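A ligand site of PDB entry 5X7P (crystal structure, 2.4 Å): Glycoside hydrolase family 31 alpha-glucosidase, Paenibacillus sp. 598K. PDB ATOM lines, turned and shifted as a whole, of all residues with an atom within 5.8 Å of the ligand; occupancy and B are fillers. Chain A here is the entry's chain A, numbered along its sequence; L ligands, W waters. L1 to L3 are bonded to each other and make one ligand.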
ATOM      1  N   ARG A 344     -36.637   1.893 -12.781  1.00  0.00           N
ATOM      2  CA  ARG A 344     -36.059   1.700 -11.426  1.00  0.00           C
ATOM      3  C   ARG A 344     -36.697   0.490 -10.762  1.00  0.00           C
ATOM      4  O   ARG A 344     -37.938   0.462 -10.628  1.00  0.00           O
ATOM      5  CB  ARG A 344     -36.404   2.862 -10.502  1.00  0.00           C
ATOM      6  CG  ARG A 344     -35.830   4.182 -10.902  1.00  0.00           C
ATOM      7  CD  ARG A 344     -34.791   4.665  -9.924  1.00  0.00           C
ATOM      8  NE  ARG A 344     -34.232   5.913 -10.421  1.00  0.00           N
ATOM      9  CZ  ARG A 344     -33.069   6.440 -10.024  1.00  0.00           C
ATOM     10  NH1 ARG A 344     -32.338   5.841  -9.088  1.00  0.00           N
ATOM     11  NH2 ARG A 344     -32.643   7.558 -10.569  1.00  0.00           N
ATOM     12  N   GLN A 349     -32.630   0.620  -8.122  1.00  0.00           N
ATOM     13  CA  GLN A 349     -31.505   0.483  -9.063  1.00  0.00           C
ATOM     14  C   GLN A 349     -31.974   0.619 -10.507  1.00  0.00           C
ATOM     15  O   GLN A 349     -32.970   0.002 -10.894  1.00  0.00           O
ATOM     16  CB  GLN A 349     -30.831  -0.890  -8.867  1.00  0.00           C
ATOM     17  CG  GLN A 349     -30.034  -1.058  -7.566  1.00  0.00           C
ATOM     18  CD  GLN A 349     -28.633  -0.439  -7.597  1.00  0.00           C
ATOM     19  OE1 GLN A 349     -27.937  -0.444  -8.620  1.00  0.00           O
ATOM     20  NE2 GLN A 349     -28.208   0.088  -6.458  1.00  0.00           N
ATOM     21  N   ARG A 350     -31.279   1.420 -11.302  1.00  0.00           N
ATOM     22  CA  ARG A 350     -31.494   1.466 -12.743  1.00  0.00           C
ATOM     23  C   ARG A 350     -31.580   0.089 -13.318  1.00  0.00           C
ATOM     24  O   ARG A 350     -30.728  -0.771 -13.038  1.00  0.00           O
ATOM     25  CB  ARG A 350     -30.359   2.192 -13.458  1.00  0.00           C
ATOM     26  CG  ARG A 350     -30.356   3.708 -13.384  1.00  0.00           C
ATOM     27  CD  ARG A 350     -31.754   4.268 -13.495  1.00  0.00           C
ATOM     28  NE  ARG A 350     -31.868   5.709 -13.738  1.00  0.00           N
ATOM     29  CZ  ARG A 350     -33.037   6.304 -14.013  1.00  0.00           C
ATOM     30  NH1 ARG A 350     -34.165   5.589 -14.031  1.00  0.00           N
ATOM     31  NH2 ARG A 350     -33.091   7.608 -14.238  1.00  0.00           N
ATOM     32  N   TYR A 354     -33.956   0.004 -18.903  1.00  0.00           N
ATOM     33  CA  TYR A 354     -33.668   1.450 -18.965  1.00  0.00           C
ATOM     34  C   TYR A 354     -32.450   1.717 -19.835  1.00  0.00           C
ATOM     35  O   TYR A 354     -32.521   2.432 -20.822  1.00  0.00           O
ATOM     36  CB  TYR A 354     -33.474   2.082 -17.557  1.00  0.00           C
ATOM     37  CG  TYR A 354     -32.859   3.470 -17.563  1.00  0.00           C
ATOM     38  CD1 TYR A 354     -33.600   4.579 -17.986  1.00  0.00           C
ATOM     39  CD2 TYR A 354     -31.528   3.690 -17.142  1.00  0.00           C
ATOM     40  CE1 TYR A 354     -33.023   5.862 -18.021  1.00  0.00           C
ATOM     41  CE2 TYR A 354     -30.955   4.960 -17.176  1.00  0.00           C
ATOM     42  CZ  TYR A 354     -31.702   6.037 -17.617  1.00  0.00           C
ATOM     43  OH  TYR A 354     -31.146   7.302 -17.664  1.00  0.00           O
ATOM     44  N   TYR A 355     -31.339   1.103 -19.474  1.00  0.00           N
ATOM     45  CA  TYR A 355     -30.085   1.314 -20.198  1.00  0.00           C
ATOM     46  C   TYR A 355     -30.278   1.017 -21.675  1.00  0.00           C
ATOM     47  O   TYR A 355     -29.874   1.822 -22.510  1.00  0.00           O
ATOM     48  CB  TYR A 355     -28.923   0.507 -19.586  1.00  0.00           C
ATOM     49  CG  TYR A 355     -28.471   1.020 -18.215  1.00  0.00           C
ATOM     50  CD1 TYR A 355     -28.165   2.376 -18.017  1.00  0.00           C
ATOM     51  CD2 TYR A 355     -28.328   0.142 -17.114  1.00  0.00           C
ATOM     52  CE1 TYR A 355     -27.776   2.852 -16.759  1.00  0.00           C
ATOM     53  CE2 TYR A 355     -27.920   0.606 -15.847  1.00  0.00           C
ATOM     54  CZ  TYR A 355     -27.644   1.967 -15.679  1.00  0.00           C
ATOM     55  OH  TYR A 355     -27.246   2.472 -14.456  1.00  0.00           O
ATOM     56  N   ASP A 358     -32.651   3.852 -23.111  1.00  0.00           N
ATOM     57  CA  ASP A 358     -32.041   5.178 -23.092  1.00  0.00           C
ATOM     58  C   ASP A 358     -30.954   5.229 -24.198  1.00  0.00           C
ATOM     59  O   ASP A 358     -31.000   6.086 -25.056  1.00  0.00           O
ATOM     60  CB  ASP A 358     -31.478   5.465 -21.686  1.00  0.00           C
ATOM     61  CG  ASP A 358     -31.035   6.903 -21.501  1.00  0.00           C
ATOM     62  OD1 ASP A 358     -31.910   7.790 -21.441  1.00  0.00           O
ATOM     63  OD2 ASP A 358     -29.804   7.147 -21.400  1.00  0.00           O
ATOM     64  N   ASP A1142     -23.867  21.239 -15.205  1.00  0.00           N
ATOM     65  CA  ASP A1142     -25.078  21.348 -14.374  1.00  0.00           C
ATOM     66  C   ASP A1142     -24.754  20.953 -12.915  1.00  0.00           C
ATOM     67  O   ASP A1142     -23.578  20.828 -12.564  1.00  0.00           O
ATOM     68  CB  ASP A1142     -26.288  20.554 -14.977  1.00  0.00           C
ATOM     69  CG  ASP A1142     -26.109  19.010 -14.956  1.00  0.00           C
ATOM     70  OD1 ASP A1142     -25.579  18.449 -13.963  1.00  0.00           O
ATOM     71  OD2 ASP A1142     -26.578  18.366 -15.937  1.00  0.00           O
ATOM     72  N   SER A1143     -25.768  20.782 -12.074  1.00  0.00           N
ATOM     73  CA  SER A1143     -25.605  20.578 -10.636  1.00  0.00           C
ATOM     74  C   SER A1143     -25.616  19.138 -10.135  1.00  0.00           C
ATOM     75  O   SER A1143     -25.313  18.891  -8.965  1.00  0.00           O
ATOM     76  CB  SER A1143     -26.712  21.338  -9.897  1.00  0.00           C
ATOM     77  OG  SER A1143     -26.620  22.727 -10.185  1.00  0.00           O
ATOM     78  N   GLY A1144     -26.029  18.192 -10.967  1.00  0.00           N
ATOM     79  CA  GLY A1144     -26.131  16.804 -10.559  1.00  0.00           C
ATOM     80  C   GLY A1144     -27.301  16.490  -9.653  1.00  0.00           C
ATOM     81  O   GLY A1144     -27.334  15.398  -9.046  1.00  0.00           O
ATOM     82  N   ALA A1146     -30.594  16.312 -10.507  1.00  0.00           N
ATOM     83  CA  ALA A1146     -31.610  15.436 -11.136  1.00  0.00           C
ATOM     84  C   ALA A1146     -31.442  13.935 -10.744  1.00  0.00           C
ATOM     85  O   ALA A1146     -32.401  13.156 -10.820  1.00  0.00           O
ATOM     86  CB  ALA A1146     -31.591  15.580 -12.666  1.00  0.00           C
ATOM     87  N   LEU A1147     -30.213  13.572 -10.362  1.00  0.00           N
ATOM     88  CA  LEU A1147     -29.853  12.201 -10.083  1.00  0.00           C
ATOM     89  C   LEU A1147     -30.231  11.847  -8.658  1.00  0.00           C
ATOM     90  O   LEU A1147     -30.204  12.667  -7.749  1.00  0.00           O
ATOM     91  CB  LEU A1147     -28.340  11.969 -10.349  1.00  0.00           C
ATOM     92  CG  LEU A1147     -27.782  12.400 -11.730  1.00  0.00           C
ATOM     93  CD1 LEU A1147     -26.269  12.524 -11.759  1.00  0.00           C
ATOM     94  CD2 LEU A1147     -28.214  11.492 -12.871  1.00  0.00           C
ATOM     95  N   HIS A1148     -30.599  10.585  -8.496  1.00  0.00           N
ATOM     96  CA  HIS A1148     -30.875   9.994  -7.212  1.00  0.00           C
ATOM     97  C   HIS A1148     -29.921   8.801  -6.927  1.00  0.00           C
ATOM     98  O   HIS A1148     -29.991   7.784  -7.611  1.00  0.00           O
ATOM     99  CB  HIS A1148     -32.304   9.505  -7.224  1.00  0.00           C
ATOM    100  CG  HIS A1148     -33.300  10.591  -7.424  1.00  0.00           C
ATOM    101  ND1 HIS A1148     -33.617  11.499  -6.428  1.00  0.00           N
ATOM    102  CD2 HIS A1148     -34.054  10.917  -8.501  1.00  0.00           C
ATOM    103  CE1 HIS A1148     -34.528  12.332  -6.894  1.00  0.00           C
ATOM    104  NE2 HIS A1148     -34.813  12.003  -8.152  1.00  0.00           N
ATOM    105  N   PRO A1149     -29.044   8.923  -5.902  1.00  0.00           N
ATOM    106  CA  PRO A1149     -28.762  10.132  -5.098  1.00  0.00           C
ATOM    107  C   PRO A1149     -28.024  11.210  -5.953  1.00  0.00           C
ATOM    108  O   PRO A1149     -27.536  10.871  -7.042  1.00  0.00           O
ATOM    109  CB  PRO A1149     -27.885   9.597  -3.955  1.00  0.00           C
ATOM    110  CG  PRO A1149     -27.256   8.360  -4.510  1.00  0.00           C
ATOM    111  CD  PRO A1149     -28.215   7.777  -5.483  1.00  0.00           C
ATOM    112  N   GLU A1151     -25.264  13.460  -7.689  1.00  0.00           N
ATOM    113  CA  GLU A1151     -23.829  13.491  -7.976  1.00  0.00           C
ATOM    114  C   GLU A1151     -23.484  14.989  -8.067  1.00  0.00           C
ATOM    115  O   GLU A1151     -23.477  15.594  -9.161  1.00  0.00           O
ATOM    116  CB  GLU A1151     -23.512  12.712  -9.276  1.00  0.00           C
ATOM    117  CG  GLU A1151     -23.329  11.194  -9.093  1.00  0.00           C
ATOM    118  CD  GLU A1151     -23.358  10.388 -10.412  1.00  0.00           C
ATOM    119  OE1 GLU A1151     -22.859  10.854 -11.476  1.00  0.00           O
ATOM    120  OE2 GLU A1151     -23.913   9.265 -10.373  1.00  0.00           O
ATOM    121  N   ARG A1159     -20.866  21.819 -11.846  1.00  0.00           N
ATOM    122  CA  ARG A1159     -19.604  21.190 -12.317  1.00  0.00           C
ATOM    123  C   ARG A1159     -19.727  20.803 -13.788  1.00  0.00           C
ATOM    124  O   ARG A1159     -20.801  20.454 -14.256  1.00  0.00           O
ATOM    125  CB  ARG A1159     -19.225  19.981 -11.435  1.00  0.00           C
ATOM    126  CG  ARG A1159     -20.031  18.702 -11.683  1.00  0.00           C
ATOM    127  CD  ARG A1159     -21.415  18.780 -11.055  1.00  0.00           C
ATOM    128  NE  ARG A1159     -22.148  17.517 -11.072  1.00  0.00           N
ATOM    129  CZ  ARG A1159     -22.762  17.005 -12.119  1.00  0.00           C
ATOM    130  NH1 ARG A1159     -22.760  17.630 -13.284  1.00  0.00           N
ATOM    131  NH2 ARG A1159     -23.413  15.859 -11.998  1.00  0.00           N
ATOM    132  N   TYR A1161     -19.362  18.170 -16.769  1.00  0.00           N
ATOM    133  CA  TYR A1161     -19.304  16.712 -16.915  1.00  0.00           C
ATOM    134  C   TYR A1161     -19.007  16.301 -18.347  1.00  0.00           C
ATOM    135  O   TYR A1161     -19.262  17.051 -19.305  1.00  0.00           O
ATOM    136  CB  TYR A1161     -20.597  16.030 -16.468  1.00  0.00           C
ATOM    137  CG  TYR A1161     -21.758  16.400 -17.351  1.00  0.00           C
ATOM    138  CD1 TYR A1161     -21.991  15.726 -18.545  1.00  0.00           C
ATOM    139  CD2 TYR A1161     -22.597  17.445 -16.999  1.00  0.00           C
ATOM    140  CE1 TYR A1161     -23.021  16.093 -19.378  1.00  0.00           C
ATOM    141  CE2 TYR A1161     -23.609  17.836 -17.827  1.00  0.00           C
ATOM    142  CZ  TYR A1161     -23.838  17.155 -19.015  1.00  0.00           C
ATOM    143  OH  TYR A1161     -24.894  17.543 -19.809  1.00  0.00           O
ATOM    144  N   HIS A1163     -20.143  12.811 -20.488  1.00  0.00           N
ATOM    145  CA  HIS A1163     -20.872  11.547 -20.458  1.00  0.00           C
ATOM    146  C   HIS A1163     -21.440  11.242 -21.802  1.00  0.00           C
ATOM    147  O   HIS A1163     -21.869  12.148 -22.519  1.00  0.00           O
ATOM    148  CB  HIS A1163     -22.012  11.560 -19.431  1.00  0.00           C
ATOM    149  CG  HIS A1163     -22.777  10.264 -19.390  1.00  0.00           C
ATOM    150  ND1 HIS A1163     -22.440   9.229 -18.540  1.00  0.00           N
ATOM    151  CD2 HIS A1163     -23.829   9.825 -20.127  1.00  0.00           C
ATOM    152  CE1 HIS A1163     -23.285   8.229 -18.725  1.00  0.00           C
ATOM    153  NE2 HIS A1163     -24.125   8.556 -19.695  1.00  0.00           N
ATOM    154  N   ASP A1165     -23.702   7.674 -23.609  1.00  0.00           N
ATOM    155  CA  ASP A1165     -24.258   6.317 -23.577  1.00  0.00           C
ATOM    156  C   ASP A1165     -23.374   5.432 -24.463  1.00  0.00           C
ATOM    157  O   ASP A1165     -23.220   4.256 -24.178  1.00  0.00           O
ATOM    158  CB  ASP A1165     -25.726   6.299 -24.131  1.00  0.00           C
ATOM    159  CG  ASP A1165     -26.772   6.913 -23.153  1.00  0.00           C
ATOM    160  OD1 ASP A1165     -26.730   6.576 -21.937  1.00  0.00           O
ATOM    161  OD2 ASP A1165     -27.633   7.707 -23.626  1.00  0.00           O
ATOM    162  N   LYS A1194     -16.454   7.958 -12.792  1.00  0.00           N
ATOM    163  CA  LYS A1194     -17.230   6.774 -12.411  1.00  0.00           C
ATOM    164  C   LYS A1194     -17.684   5.983 -13.612  1.00  0.00           C
ATOM    165  O   LYS A1194     -17.563   6.448 -14.780  1.00  0.00           O
ATOM    166  CB  LYS A1194     -18.372   7.127 -11.429  1.00  0.00           C
ATOM    167  CG  LYS A1194     -19.594   7.829 -11.976  1.00  0.00           C
ATOM    168  CD  LYS A1194     -19.973   9.042 -11.121  1.00  0.00           C
ATOM    169  CE  LYS A1194     -20.338   8.734  -9.662  1.00  0.00           C
ATOM    170  NZ  LYS A1194     -21.410   7.715  -9.501  1.00  0.00           N
ATOM    171  N   ASN A1195     -18.132   4.751 -13.294  1.00  0.00           N
ATOM    172  CA  ASN A1195     -18.600   3.761 -14.271  1.00  0.00           C
ATOM    173  C   ASN A1195     -17.445   3.299 -15.162  1.00  0.00           C
ATOM    174  O   ASN A1195     -16.394   3.004 -14.631  1.00  0.00           O
ATOM    175  CB  ASN A1195     -19.815   4.307 -15.012  1.00  0.00           C
ATOM    176  CG  ASN A1195     -20.933   4.663 -14.053  1.00  0.00           C
ATOM    177  OD1 ASN A1195     -21.113   3.999 -13.018  1.00  0.00           O
ATOM    178  ND2 ASN A1195     -21.677   5.723 -14.369  1.00  0.00           N
ATOM    179  N   THR A1251     -18.374   8.433 -16.982  1.00  0.00           N
ATOM    180  CA  THR A1251     -18.740   9.765 -16.516  1.00  0.00           C
ATOM    181  C   THR A1251     -17.551  10.448 -15.808  1.00  0.00           C
ATOM    182  O   THR A1251     -16.951   9.897 -14.884  1.00  0.00           O
ATOM    183  CB  THR A1251     -19.934   9.729 -15.573  1.00  0.00           C
ATOM    184  OG1 THR A1251     -21.020   9.047 -16.213  1.00  0.00           O
ATOM    185  CG2 THR A1251     -20.331  11.145 -15.203  1.00  0.00           C
ATOM    186  N   HIS A1253     -16.529  14.099 -13.962  1.00  0.00           N
ATOM    187  CA  HIS A1253     -16.885  15.427 -13.455  1.00  0.00           C
ATOM    188  C   HIS A1253     -15.629  16.232 -13.189  1.00  0.00           C
ATOM    189  O   HIS A1253     -14.693  15.726 -12.566  1.00  0.00           O
ATOM    190  CB  HIS A1253     -17.719  15.343 -12.145  1.00  0.00           C
ATOM    191  CG  HIS A1253     -18.991  14.591 -12.306  1.00  0.00           C
ATOM    192  ND1 HIS A1253     -19.346  13.539 -11.498  1.00  0.00           N
ATOM    193  CD2 HIS A1253     -19.971  14.700 -13.231  1.00  0.00           C
ATOM    194  CE1 HIS A1253     -20.509  13.059 -11.888  1.00  0.00           C
ATOM    195  NE2 HIS A1253     -20.914  13.744 -12.937  1.00  0.00           N
HETATM  196  O1  LIG L   1     -27.977   7.323  -9.810  1.00  0.00           O
HETATM  197  C1  LG2 L   2     -28.485   6.274 -10.624  1.00  0.00           C
HETATM  198  C2  LG2 L   2     -27.367   5.312 -11.072  1.00  0.00           C
HETATM  199  C3  LG2 L   2     -26.351   6.077 -11.914  1.00  0.00           C
HETATM  200  C4  LG2 L   2     -27.044   6.792 -13.072  1.00  0.00           C
HETATM  201  C5  LG2 L   2     -28.330   7.569 -12.706  1.00  0.00           C
HETATM  202  C6  LG2 L   2     -29.132   7.853 -13.994  1.00  0.00           C
HETATM  203  O1  LG2 L   2     -26.671   4.690  -9.983  1.00  0.00           O
HETATM  204  O2  LG2 L   2     -25.334   5.200 -12.408  1.00  0.00           O
HETATM  205  O3  LG2 L   2     -26.100   7.769 -13.504  1.00  0.00           O
HETATM  206  O4  LG2 L   2     -29.167   6.911 -11.735  1.00  0.00           O
HETATM  207  O5  LG2 L   2     -30.032   8.973 -13.850  1.00  0.00           O
HETATM  208  C1  LG3 L   3     -25.268   7.536 -14.640  1.00  0.00           C
HETATM  209  O1  LG3 L   3     -23.366   8.074 -13.108  1.00  0.00           O
HETATM  210  C2  LG3 L   3     -24.016   8.374 -14.365  1.00  0.00           C
HETATM  211  C3  LG3 L   3     -25.804  15.226 -16.797  1.00  0.00           C
HETATM  212  C4  LG3 L   3     -24.458   9.837 -14.346  1.00  0.00           C
HETATM  213  O2  LG3 L   3     -23.364  10.661 -13.965  1.00  0.00           O
HETATM  214  C5  LG3 L   3     -25.036  10.218 -15.702  1.00  0.00           C
HETATM  215  N1  LG3 L   3     -25.321  11.638 -15.677  1.00  0.00           N
HETATM  216  C6  LG3 L   3     -26.283   9.358 -16.006  1.00  0.00           C
HETATM  217  O3  LG3 L   3     -25.916   7.959 -15.880  1.00  0.00           O
HETATM  218  C7  LG3 L   3     -26.946   9.629 -17.375  1.00  0.00           C
HETATM  219  C8  LG3 L   3     -24.424  12.594 -16.328  1.00  0.00           C
HETATM  220  C9  LG3 L   3     -24.077  13.857 -15.489  1.00  0.00           C
HETATM  221  O4  LG3 L   3     -23.576  13.615 -14.124  1.00  0.00           O
HETATM  222  C10 LG3 L   3     -25.258  14.815 -15.413  1.00  0.00           C
HETATM  223  O5  LG3 L   3     -24.760  15.967 -14.713  1.00  0.00           O
HETATM  224  O6  LG3 L   3     -27.169  15.657 -16.718  1.00  0.00           O
HETATM  225  C11 LG3 L   3     -25.650  14.145 -17.878  1.00  0.00           C
HETATM  226  C12 LG3 L   3     -25.043  12.955 -17.656  1.00  0.00           C
HETATM  227  C13 LG3 L   3     -26.144  14.444 -19.291  1.00  0.00           C
HETATM  228  O7  LG3 L   3     -26.885  13.348 -19.809  1.00  0.00           O
HETATM  229  O   HOH W   1     -26.559   8.928  -8.673  1.00  0.00           O
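The guanidinium group (NH2) of Arg 350 sits at hydrogen-bond distance from an oxygen (O5) of LG2 L2. O of His 1148 sits at hydrogen-bond distance from O1 of LIG L1, at 3.0 Å. An oxygen (O5) of LG3 L3 is in hydrogen-bond range of the guanidinium group (NH1) of Arg 1159, 3.0 Å away. O4 of LG3 L3 sits at hydrogen-bond distance from NE2 of His 1253. The side-chain carboxylate (OE1) of Glu 1151 lies within hydrogen-bond range of an oxygen (O2) of LG3 L3, 2.5 Å away. An oxygen (O5) of LG3 L3 lies within hydrogen-bond range of the side-chain carboxylate of Asp 1142, 2.7 Å away. ND2 of Asn 1195 is in hydrogen-bond range of O1 of LG3 L3 (3.2 Å).
Water W1 lies within hydrogen-bond range of an oxygen (O1) of LIG L1, the backbone carbonyl oxygen of Pro 1149 and the side-chain carboxylate of Glu 1151.
NH1 of Arg 1159 is in salt-bridge range of OD1 of Asp 1142 (3.0 Å). ND1 of His 1163 lies within hydrogen-bond range of OG1 of Thr 1251 (2.7 Å). The side-chain carboxylate (OE2) of Glu 1151 is in salt-bridge range of the side-chain amino group (NZ) of Lys 1194, at 3.1 Å. The backbone carbonyl oxygen (O) of Glu 1151 sits at hydrogen-bond distance from the guanidinium group (NH2) of Arg 1159. A ring nitrogen (NE2) of His 1253 sits at hydrogen-bond distance from the guanidinium group (NH2) of Arg 1159. O of Thr 1251 sits at hydrogen-bond distance from N of Lys 1194 (2.9 Å). The backbone NH of Glu 1151 lies within hydrogen-bond range of the backbone carbonyl oxygen of Gly 1144, 3.1 Å away. The side-chain carboxylate of Asp 1142 is in hydrogen-bond range of the backbone NH of Gly 1144 (3.0 Å).
Merely in contact with the ligand: Leu 1147 (3.3 Å), Thr 1251 (3.3 Å), Tyr 1161 (3.4 Å), Arg 344 (3.7 Å), His 1163 (3.8 Å), Tyr 355 (3.9 Å) and Lys 1194 (3.9 Å). Hydrophobic or aromatic side chains within 4 Å of the ligand: Leu 1147, Tyr 1161, His 1163 and His 1253. 14 residues have an atom within 4 Å of the ligand: Arg 344, Arg 350, Tyr 355, Asp 1142, Leu 1147, His 1148, Glu 1151, Arg 1159, Tyr 1161, His 1163, Lys 1194, Asn 1195, Thr 1251 and His 1253. The nearest printed residue that does not touch the ligand is Tyr 354 (4.2 Å).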
